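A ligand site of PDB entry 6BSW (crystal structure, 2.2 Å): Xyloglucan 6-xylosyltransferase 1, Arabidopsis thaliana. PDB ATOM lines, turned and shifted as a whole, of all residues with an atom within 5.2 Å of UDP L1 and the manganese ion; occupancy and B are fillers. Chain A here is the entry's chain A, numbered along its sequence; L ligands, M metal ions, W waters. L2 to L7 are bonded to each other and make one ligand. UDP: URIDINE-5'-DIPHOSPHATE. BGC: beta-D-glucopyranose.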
ATOM      1  N   THR A  40      19.533 -18.315  -3.552  1.00  0.00           N
ATOM      2  CA  THR A  40      19.688 -19.741  -3.800  1.00  0.00           C
ATOM      3  C   THR A  40      20.743 -19.914  -4.890  1.00  0.00           C
ATOM      4  O   THR A  40      21.324 -18.941  -5.374  1.00  0.00           O
ATOM      5  CB  THR A  40      18.350 -20.384  -4.176  1.00  0.00           C
ATOM      6  OG1 THR A  40      18.522 -21.788  -4.367  1.00  0.00           O
ATOM      7  CG2 THR A  40      17.795 -19.764  -5.452  1.00  0.00           C
ATOM      8  N   GLY A  41      20.990 -21.161  -5.274  1.00  0.00           N
ATOM      9  CA  GLY A  41      21.979 -21.404  -6.310  1.00  0.00           C
ATOM     10  C   GLY A  41      22.152 -22.887  -6.566  1.00  0.00           C
ATOM     11  O   GLY A  41      21.640 -23.738  -5.825  1.00  0.00           O
ATOM     12  N   SER A  42      22.891 -23.176  -7.633  1.00  0.00           N
ATOM     13  CA  SER A  42      23.206 -24.542  -8.032  1.00  0.00           C
ATOM     14  C   SER A  42      24.453 -24.516  -8.896  1.00  0.00           C
ATOM     15  O   SER A  42      24.892 -23.461  -9.351  1.00  0.00           O
ATOM     16  CB  SER A  42      22.028 -25.189  -8.781  1.00  0.00           C
ATOM     17  OG  SER A  42      21.648 -24.415  -9.894  1.00  0.00           O
ATOM     18  N   ALA A  43      25.034 -25.698  -9.106  1.00  0.00           N
ATOM     19  CA  ALA A  43      26.286 -25.798  -9.827  1.00  0.00           C
ATOM     20  C   ALA A  43      26.102 -25.306 -11.270  1.00  0.00           C
ATOM     21  O   ALA A  43      25.038 -25.505 -11.871  1.00  0.00           O
ATOM     22  CB  ALA A  43      26.803 -27.233  -9.817  1.00  0.00           C
ATOM     23  N   GLY A  87      31.091 -26.885  -3.528  1.00  0.00           N
ATOM     24  CA  GLY A  87      29.979 -27.626  -2.977  1.00  0.00           C
ATOM     25  C   GLY A  87      29.047 -26.779  -2.138  1.00  0.00           C
ATOM     26  O   GLY A  87      28.786 -25.617  -2.466  1.00  0.00           O
ATOM     27  N   PHE A  88      28.542 -27.350  -1.044  1.00  0.00           N
ATOM     28  CA  PHE A  88      27.642 -26.613  -0.157  1.00  0.00           C
ATOM     29  C   PHE A  88      28.362 -25.511   0.618  1.00  0.00           C
ATOM     30  O   PHE A  88      27.686 -24.699   1.254  1.00  0.00           O
ATOM     31  CB  PHE A  88      26.927 -27.549   0.826  1.00  0.00           C
ATOM     32  CG  PHE A  88      27.747 -28.712   1.286  1.00  0.00           C
ATOM     33  CD1 PHE A  88      28.908 -28.524   2.013  1.00  0.00           C
ATOM     34  CD2 PHE A  88      27.348 -30.010   0.995  1.00  0.00           C
ATOM     35  CE1 PHE A  88      29.665 -29.604   2.439  1.00  0.00           C
ATOM     36  CE2 PHE A  88      28.092 -31.091   1.424  1.00  0.00           C
ATOM     37  CZ  PHE A  88      29.255 -30.886   2.136  1.00  0.00           C
ATOM     38  N   ALA A  90      29.979 -23.209  -0.934  1.00  0.00           N
ATOM     39  CA  ALA A  90      30.047 -22.087  -1.864  1.00  0.00           C
ATOM     40  C   ALA A  90      29.169 -20.915  -1.433  1.00  0.00           C
ATOM     41  O   ALA A  90      29.338 -19.805  -1.948  1.00  0.00           O
ATOM     42  CB  ALA A  90      29.640 -22.532  -3.268  1.00  0.00           C
ATOM     43  N   LYS A  91      28.238 -21.130  -0.508  1.00  0.00           N
ATOM     44  CA  LYS A  91      27.326 -20.064  -0.116  1.00  0.00           C
ATOM     45  C   LYS A  91      27.953 -19.059   0.831  1.00  0.00           C
ATOM     46  O   LYS A  91      27.438 -17.937   0.951  1.00  0.00           O
ATOM     47  CB  LYS A  91      26.049 -20.638   0.501  1.00  0.00           C
ATOM     48  CG  LYS A  91      26.264 -21.613   1.648  1.00  0.00           C
ATOM     49  CD  LYS A  91      24.943 -22.287   2.001  1.00  0.00           C
ATOM     50  CE  LYS A  91      25.143 -23.411   3.012  1.00  0.00           C
ATOM     51  NZ  LYS A  91      23.899 -24.211   3.198  1.00  0.00           N
ATOM     52  N   TRP A 110      18.969 -17.185   2.730  1.00  0.00           N
ATOM     53  CA  TRP A 110      19.472 -18.285   1.926  1.00  0.00           C
ATOM     54  C   TRP A 110      18.454 -19.421   1.941  1.00  0.00           C
ATOM     55  O   TRP A 110      17.843 -19.723   2.971  1.00  0.00           O
ATOM     56  CB  TRP A 110      20.805 -18.790   2.447  1.00  0.00           C
ATOM     57  CG  TRP A 110      21.181 -20.096   1.806  1.00  0.00           C
ATOM     58  CD1 TRP A 110      21.016 -21.345   2.331  1.00  0.00           C
ATOM     59  CD2 TRP A 110      21.755 -20.279   0.504  1.00  0.00           C
ATOM     60  NE1 TRP A 110      21.463 -22.293   1.435  1.00  0.00           N
ATOM     61  CE2 TRP A 110      21.916 -21.661   0.309  1.00  0.00           C
ATOM     62  CE3 TRP A 110      22.146 -19.393  -0.510  1.00  0.00           C
ATOM     63  CZ2 TRP A 110      22.453 -22.186  -0.860  1.00  0.00           C
ATOM     64  CZ3 TRP A 110      22.677 -19.924  -1.673  1.00  0.00           C
ATOM     65  CH2 TRP A 110      22.831 -21.306  -1.841  1.00  0.00           C
ATOM     66  N   MET A 111      18.292 -20.078   0.783  1.00  0.00           N
ATOM     67  CA  MET A 111      17.380 -21.200   0.667  1.00  0.00           C
ATOM     68  C   MET A 111      17.961 -22.211  -0.314  1.00  0.00           C
ATOM     69  O   MET A 111      18.259 -21.857  -1.461  1.00  0.00           O
ATOM     70  CB  MET A 111      15.991 -20.747   0.197  1.00  0.00           C
ATOM     71  CG  MET A 111      14.926 -21.800   0.358  1.00  0.00           C
ATOM     72  SD  MET A 111      13.265 -21.121   0.210  1.00  0.00           S
ATOM     73  CE  MET A 111      12.282 -22.610   0.409  1.00  0.00           C
ATOM     74  N   ASP A 112      18.107 -23.446   0.143  1.00  0.00           N
ATOM     75  CA  ASP A 112      18.630 -24.521  -0.685  1.00  0.00           C
ATOM     76  C   ASP A 112      17.787 -24.713  -1.950  1.00  0.00           C
ATOM     77  O   ASP A 112      16.601 -24.387  -2.003  1.00  0.00           O
ATOM     78  CB  ASP A 112      18.659 -25.830   0.099  1.00  0.00           C
ATOM     79  CG  ASP A 112      19.949 -26.036   0.861  1.00  0.00           C
ATOM     80  OD1 ASP A 112      20.707 -25.060   1.029  1.00  0.00           O
ATOM     81  OD2 ASP A 112      20.201 -27.183   1.282  1.00  0.00           O
ATOM     82  N   SER A 113      18.432 -25.263  -2.983  1.00  0.00           N
ATOM     83  CA  SER A 113      17.723 -25.541  -4.222  1.00  0.00           C
ATOM     84  C   SER A 113      16.770 -26.726  -4.084  1.00  0.00           C
ATOM     85  O   SER A 113      15.776 -26.806  -4.820  1.00  0.00           O
ATOM     86  CB  SER A 113      18.711 -25.801  -5.361  1.00  0.00           C
ATOM     87  OG  SER A 113      19.439 -26.989  -5.142  1.00  0.00           O
ATOM     88  N   ASP A 114      17.048 -27.646  -3.162  1.00  0.00           N
ATOM     89  CA  ASP A 114      16.145 -28.758  -2.869  1.00  0.00           C
ATOM     90  C   ASP A 114      15.123 -28.400  -1.794  1.00  0.00           C
ATOM     91  O   ASP A 114      14.496 -29.299  -1.220  1.00  0.00           O
ATOM     92  CB  ASP A 114      16.933 -30.010  -2.462  1.00  0.00           C
ATOM     93  CG  ASP A 114      17.741 -29.817  -1.193  1.00  0.00           C
ATOM     94  OD1 ASP A 114      18.262 -28.706  -0.973  1.00  0.00           O
ATOM     95  OD2 ASP A 114      17.873 -30.786  -0.418  1.00  0.00           O
ATOM     96  N   HIS A 262      11.820 -29.547   2.553  1.00  0.00           N
ATOM     97  CA  HIS A 262      13.230 -29.591   2.182  1.00  0.00           C
ATOM     98  C   HIS A 262      13.626 -31.041   1.985  1.00  0.00           C
ATOM     99  O   HIS A 262      13.528 -31.847   2.917  1.00  0.00           O
ATOM    100  CB  HIS A 262      14.093 -28.904   3.256  1.00  0.00           C
ATOM    101  CG  HIS A 262      15.534 -28.781   2.886  1.00  0.00           C
ATOM    102  ND1 HIS A 262      16.478 -28.258   3.757  1.00  0.00           N
ATOM    103  CD2 HIS A 262      16.202 -29.106   1.755  1.00  0.00           C
ATOM    104  CE1 HIS A 262      17.659 -28.278   3.177  1.00  0.00           C
ATOM    105  NE2 HIS A 262      17.530 -28.776   1.961  1.00  0.00           N
ATOM    106  N   PHE A 263      14.088 -31.374   0.784  1.00  0.00           N
ATOM    107  CA  PHE A 263      14.357 -32.762   0.422  1.00  0.00           C
ATOM    108  C   PHE A 263      15.826 -33.115   0.694  1.00  0.00           C
ATOM    109  O   PHE A 263      16.583 -33.538  -0.173  1.00  0.00           O
ATOM    110  CB  PHE A 263      13.966 -33.009  -1.031  1.00  0.00           C
ATOM    111  CG  PHE A 263      12.487 -33.015  -1.250  1.00  0.00           C
ATOM    112  CD1 PHE A 263      11.799 -31.833  -1.456  1.00  0.00           C
ATOM    113  CD2 PHE A 263      11.766 -34.198  -1.211  1.00  0.00           C
ATOM    114  CE1 PHE A 263      10.437 -31.823  -1.640  1.00  0.00           C
ATOM    115  CE2 PHE A 263      10.398 -34.194  -1.389  1.00  0.00           C
ATOM    116  CZ  PHE A 263       9.728 -33.010  -1.612  1.00  0.00           C
ATOM    117  N   VAL A 264      16.197 -32.944   1.964  1.00  0.00           N
ATOM    118  CA  VAL A 264      17.540 -33.293   2.419  1.00  0.00           C
ATOM    119  C   VAL A 264      17.819 -34.763   2.150  1.00  0.00           C
ATOM    120  O   VAL A 264      16.960 -35.629   2.350  1.00  0.00           O
ATOM    121  CB  VAL A 264      17.696 -32.958   3.911  1.00  0.00           C
ATOM    122  CG1 VAL A 264      17.582 -31.463   4.149  1.00  0.00           C
ATOM    123  CG2 VAL A 264      16.653 -33.718   4.741  1.00  0.00           C
ATOM    124  N   GLY A 265      19.040 -35.051   1.695  1.00  0.00           N
ATOM    125  CA  GLY A 265      19.466 -36.407   1.455  1.00  0.00           C
ATOM    126  C   GLY A 265      19.074 -36.987   0.108  1.00  0.00           C
ATOM    127  O   GLY A 265      19.498 -38.101  -0.202  1.00  0.00           O
ATOM    128  N   CYS A 266      18.304 -36.253  -0.694  1.00  0.00           N
ATOM    129  CA  CYS A 266      17.789 -36.793  -1.953  1.00  0.00           C
ATOM    130  C   CYS A 266      18.764 -36.606  -3.108  1.00  0.00           C
ATOM    131  O   CYS A 266      18.943 -37.528  -3.923  1.00  0.00           O
ATOM    132  CB  CYS A 266      16.449 -36.145  -2.277  1.00  0.00           C
ATOM    133  SG  CYS A 266      15.045 -36.940  -1.445  1.00  0.00           S
ATOM    134  N   LYS A 267      19.390 -35.446  -3.219  1.00  0.00           N
ATOM    135  CA  LYS A 267      20.340 -35.195  -4.293  1.00  0.00           C
ATOM    136  C   LYS A 267      19.679 -35.385  -5.651  1.00  0.00           C
ATOM    137  O   LYS A 267      20.136 -36.216  -6.450  1.00  0.00           O
ATOM    138  CB  LYS A 267      21.562 -36.113  -4.172  1.00  0.00           C
ATOM    139  CG  LYS A 267      22.247 -36.077  -2.820  1.00  0.00           C
ATOM    140  CD  LYS A 267      22.545 -34.646  -2.390  1.00  0.00           C
ATOM    141  CE  LYS A 267      23.273 -34.589  -1.062  1.00  0.00           C
ATOM    142  NZ  LYS A 267      23.165 -33.237  -0.444  1.00  0.00           N
HETATM  143  N1  UDP L   1      24.925 -25.714  -3.937  1.00  0.00           N
HETATM  144  C2  UDP L   1      25.598 -24.663  -4.735  1.00  0.00           C
HETATM  145  N3  UDP L   1      26.725 -25.046  -5.661  1.00  0.00           N
HETATM  146  C4  UDP L   1      27.160 -26.423  -5.780  1.00  0.00           C
HETATM  147  C5  UDP L   1      26.479 -27.480  -4.963  1.00  0.00           C
HETATM  148  C6  UDP L   1      25.369 -27.096  -4.054  1.00  0.00           C
HETATM  149  O2  UDP L   1      25.257 -23.549  -4.658  1.00  0.00           O
HETATM  150  O4  UDP L   1      28.055 -26.693  -6.518  1.00  0.00           O
HETATM  151  C1' UDP L   1      23.944 -25.364  -3.123  1.00  0.00           C
HETATM  152  C2' UDP L   1      22.588 -25.960  -3.549  1.00  0.00           C
HETATM  153  O2' UDP L   1      21.531 -24.973  -3.318  1.00  0.00           O
HETATM  154  C3' UDP L   1      22.422 -27.008  -2.746  1.00  0.00           C
HETATM  155  C4' UDP L   1      23.147 -26.585  -1.341  1.00  0.00           C
HETATM  156  O4' UDP L   1      24.231 -25.930  -1.685  1.00  0.00           O
HETATM  157  O3' UDP L   1      21.040 -27.270  -2.504  1.00  0.00           O
HETATM  158  C5' UDP L   1      23.498 -27.806  -0.571  1.00  0.00           C
HETATM  159  O5' UDP L   1      22.311 -28.407  -0.141  1.00  0.00           O
HETATM  160  PA  UDP L   1      22.039 -30.022  -0.369  1.00  0.00           P
HETATM  161  O1A UDP L   1      22.879 -30.586  -1.483  1.00  0.00           O
HETATM  162  O2A UDP L   1      20.567 -30.191  -0.702  1.00  0.00           O
HETATM  163  O3A UDP L   1      22.388 -30.827   1.024  1.00  0.00           O
HETATM  164  PB  UDP L   1      21.211 -31.610   1.865  1.00  0.00           P
HETATM  165  O1B UDP L   1      21.797 -32.168   3.149  1.00  0.00           O
HETATM  166  O2B UDP L   1      20.129 -30.582   2.169  1.00  0.00           O
HETATM  167  O3B UDP L   1      20.669 -32.739   0.996  1.00  0.00           O
HETATM  168  C2  BGC L   2       8.924 -32.493  17.312  1.00  0.00           C
HETATM  169  C3  BGC L   2       9.766 -33.561  16.721  1.00  0.00           C
HETATM  170  C4  BGC L   2      11.234 -33.275  16.853  1.00  0.00           C
HETATM  171  C5  BGC L   2      11.609 -32.978  18.293  1.00  0.00           C
HETATM  172  C6  BGC L   2      13.065 -32.608  18.383  1.00  0.00           C
HETATM  173  C1  BGC L   2       9.332 -32.147  18.732  1.00  0.00           C
HETATM  174  O1  BGC L   2       8.646 -31.050  19.133  1.00  0.00           O
HETATM  175  O2  BGC L   2       7.538 -32.937  17.326  1.00  0.00           O
HETATM  176  O3  BGC L   2       9.424 -33.689  15.319  1.00  0.00           O
HETATM  177  O4  BGC L   2      11.979 -34.424  16.396  1.00  0.00           O
HETATM  178  O5  BGC L   2      10.809 -31.860  18.837  1.00  0.00           O
HETATM  179  O6  BGC L   2      13.321 -32.050  19.636  1.00  0.00           O
HETATM  180  C2  BGC L   3      13.905 -35.238  15.259  1.00  0.00           C
HETATM  181  C3  BGC L   3      14.914 -34.955  14.202  1.00  0.00           C
HETATM  182  C4  BGC L   3      14.353 -34.381  12.940  1.00  0.00           C
HETATM  183  C5  BGC L   3      13.317 -33.274  13.198  1.00  0.00           C
HETATM  184  C6  BGC L   3      12.620 -32.906  11.904  1.00  0.00           C
HETATM  185  C1  BGC L   3      12.953 -34.063  15.476  1.00  0.00           C
HETATM  186  O2  BGC L   3      14.601 -35.493  16.485  1.00  0.00           O
HETATM  187  O3  BGC L   3      15.595 -36.201  13.860  1.00  0.00           O
HETATM  188  O4  BGC L   3      15.454 -33.814  12.196  1.00  0.00           O
HETATM  189  O5  BGC L   3      12.305 -33.665  14.189  1.00  0.00           O
HETATM  190  O6  BGC L   3      11.853 -31.725  12.103  1.00  0.00           O
HETATM  191  C2  BGC L   4      16.454 -33.378  10.137  1.00  0.00           C
HETATM  192  C3  BGC L   4      16.872 -33.916   8.799  1.00  0.00           C
HETATM  193  C4  BGC L   4      17.373 -35.315   8.885  1.00  0.00           C
HETATM  194  C5  BGC L   4      16.348 -36.214   9.567  1.00  0.00           C
HETATM  195  C6  BGC L   4      16.851 -37.636   9.646  1.00  0.00           C
HETATM  196  C1  BGC L   4      15.549 -34.309  10.908  1.00  0.00           C
HETATM  197  O2  BGC L   4      15.742 -32.146   9.945  1.00  0.00           O
HETATM  198  O3  BGC L   4      17.918 -33.065   8.272  1.00  0.00           O
HETATM  199  O4  BGC L   4      17.650 -35.819   7.526  1.00  0.00           O
HETATM  200  O5  BGC L   4      16.061 -35.722  10.938  1.00  0.00           O
HETATM  201  O6  BGC L   4      18.150 -37.655  10.172  1.00  0.00           O
HETATM  202  C2  BGC L   5      19.339 -36.526   6.006  1.00  0.00           C
HETATM  203  C3  BGC L   5      20.767 -36.419   5.573  1.00  0.00           C
HETATM  204  C4  BGC L   5      21.198 -35.018   5.407  1.00  0.00           C
HETATM  205  C5  BGC L   5      20.937 -34.211   6.709  1.00  0.00           C
HETATM  206  C6  BGC L   5      21.276 -32.852   6.538  1.00  0.00           C
HETATM  207  C1  BGC L   5      19.058 -35.754   7.235  1.00  0.00           C
HETATM  208  O2  BGC L   5      19.021 -37.944   6.235  1.00  0.00           O
HETATM  209  O3  BGC L   5      20.858 -37.188   4.316  1.00  0.00           O
HETATM  210  O4  BGC L   5      22.635 -34.843   5.139  1.00  0.00           O
HETATM  211  O5  BGC L   5      19.431 -34.349   7.074  1.00  0.00           O
HETATM  212  O6  BGC L   5      20.627 -32.319   5.376  1.00  0.00           O
HETATM  213  C2  BGC L   6      24.325 -35.008   3.495  1.00  0.00           C
HETATM  214  C3  BGC L   6      25.148 -35.894   2.638  1.00  0.00           C
HETATM  215  C4  BGC L   6      25.647 -37.105   3.327  1.00  0.00           C
HETATM  216  C5  BGC L   6      24.528 -37.883   4.105  1.00  0.00           C
HETATM  217  C6  BGC L   6      25.112 -38.865   4.957  1.00  0.00           C
HETATM  218  C1  BGC L   6      23.235 -35.727   4.207  1.00  0.00           C
HETATM  219  O2  BGC L   6      23.727 -33.993   2.631  1.00  0.00           O
HETATM  220  O3  BGC L   6      26.323 -35.105   2.158  1.00  0.00           O
HETATM  221  O4  BGC L   6      26.177 -37.995   2.344  1.00  0.00           O
HETATM  222  O5  BGC L   6      23.730 -36.883   4.968  1.00  0.00           O
HETATM  223  O6  BGC L   6      24.075 -39.499   5.721  1.00  0.00           O
HETATM  224  C2  BGC L   7      28.034 -39.288   1.694  1.00  0.00           C
HETATM  225  C3  BGC L   7      29.475 -39.295   1.288  1.00  0.00           C
HETATM  226  C4  BGC L   7      29.774 -38.196   0.333  1.00  0.00           C
HETATM  227  C5  BGC L   7      29.357 -36.848   0.879  1.00  0.00           C
HETATM  228  C6  BGC L   7      29.587 -35.804  -0.178  1.00  0.00           C
HETATM  229  C1  BGC L   7      27.579 -37.940   2.207  1.00  0.00           C
HETATM  230  O2  BGC L   7      27.850 -40.257   2.735  1.00  0.00           O
HETATM  231  O3  BGC L   7      29.774 -40.565   0.654  1.00  0.00           O
HETATM  232  O4  BGC L   7      31.191 -38.181   0.082  1.00  0.00           O
HETATM  233  O5  BGC L   7      27.922 -36.828   1.287  1.00  0.00           O
HETATM  234  O6  BGC L   7      28.881 -34.638   0.142  1.00  0.00           O
HETATM  235 MN    MN M   1      19.322 -29.096   0.786  1.00  0.00          MN
HETATM  236  O   HOH W   1      19.337 -32.993  -1.274  1.00  0.00           O
HETATM  237  O   HOH W   2      20.831 -31.529  -3.172  1.00  0.00           O
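The side-chain amino group (NZ) of Lys 267 sits at hydrogen-bond distance from an oxygen (O2) of BGC L6, at 3.2 Å.
The backbone NH (N) of Ser 113 is in hydrogen-bond range of an oxygen (O2') of UDP L1, 3.1 Å away.
An oxygen (O3') of UDP L1 sits at hydrogen-bond distance from the side-chain hydroxyl of Ser 113 (3.1 Å).
The backbone carbonyl oxygen of Gly 41 is in hydrogen-bond range of an oxygen (O2') of UDP L1, 2.8 Å away.
An oxygen (O1A) of UDP L1 lies within salt-bridge range of the side-chain amino group (NZ) of Lys 267.
An oxygen (O3B) of UDP L1 is in hydrogen-bond range of the backbone NH (N) of Gly 265.
O6 of BGC L5 sits at hydrogen-bond distance from O1B of UDP L1 (2.5 Å).
The manganese ion is bound by the side-chain carboxylate (OD1) of Asp 114 (2.1 Å), the side-chain carboxylate (OD2) of Asp 112 (2.2 Å), a ring nitrogen (NE2) of His 262 (2.2 Å), an oxygen (O2B) of UDP L1 (2.2 Å), an oxygen (O2A) of UDP L1 (2.2 Å) and the side-chain carboxylate (OD2) of Asp 114 (2.5 Å).
The manganese ion has six donor atoms within binding distance.
The side-chain carboxylate (OD1) of Asp 112 lies within hydrogen-bond range of the indole nitrogen (NE1) of Trp 110 (2.9 Å).
O of Asp 114 sits at hydrogen-bond distance from N of Phe 263, 2.9 Å away.
The side-chain carboxylate (OD1) of Asp 112 lies within salt-bridge range of the side-chain amino group (NZ) of Lys 91, at 3.95 Å.
Within 4 Å of the manganese ion: Asp 112, Asp 114 and His 262.
N of Ser 42 touches O2 of UDP L1, 3.8 Å away.
CB of Ala 43 touches O4 of UDP L1 (3.6 Å).
Gly 87 touches UDP L1 (O to C4, 3.8 Å).
Phe 88 touches UDP L1 (CB to C5', 3.7 Å).
Trp 110 touches UDP L1.
Val 264 touches UDP L1 (CG1 to O2B, 3.3 Å).
Within 4 Å of UDP L1: Gly 41, Ser 42, Ala 43, Gly 87, Phe 88, Trp 110, Asp 112, Ser 113, Asp 114, His 262, Val 264, Gly 265 and Lys 267.
The nearest printed residue that does not touch UDP L1 is Phe 263 (4.3 Å).
Water W1 lies within hydrogen-bond range of an oxygen (O3B) of UDP L1, the backbone carbonyl oxygen of Phe 263, the backbone NH of Lys 267 and the backbone NH of Cys 266.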
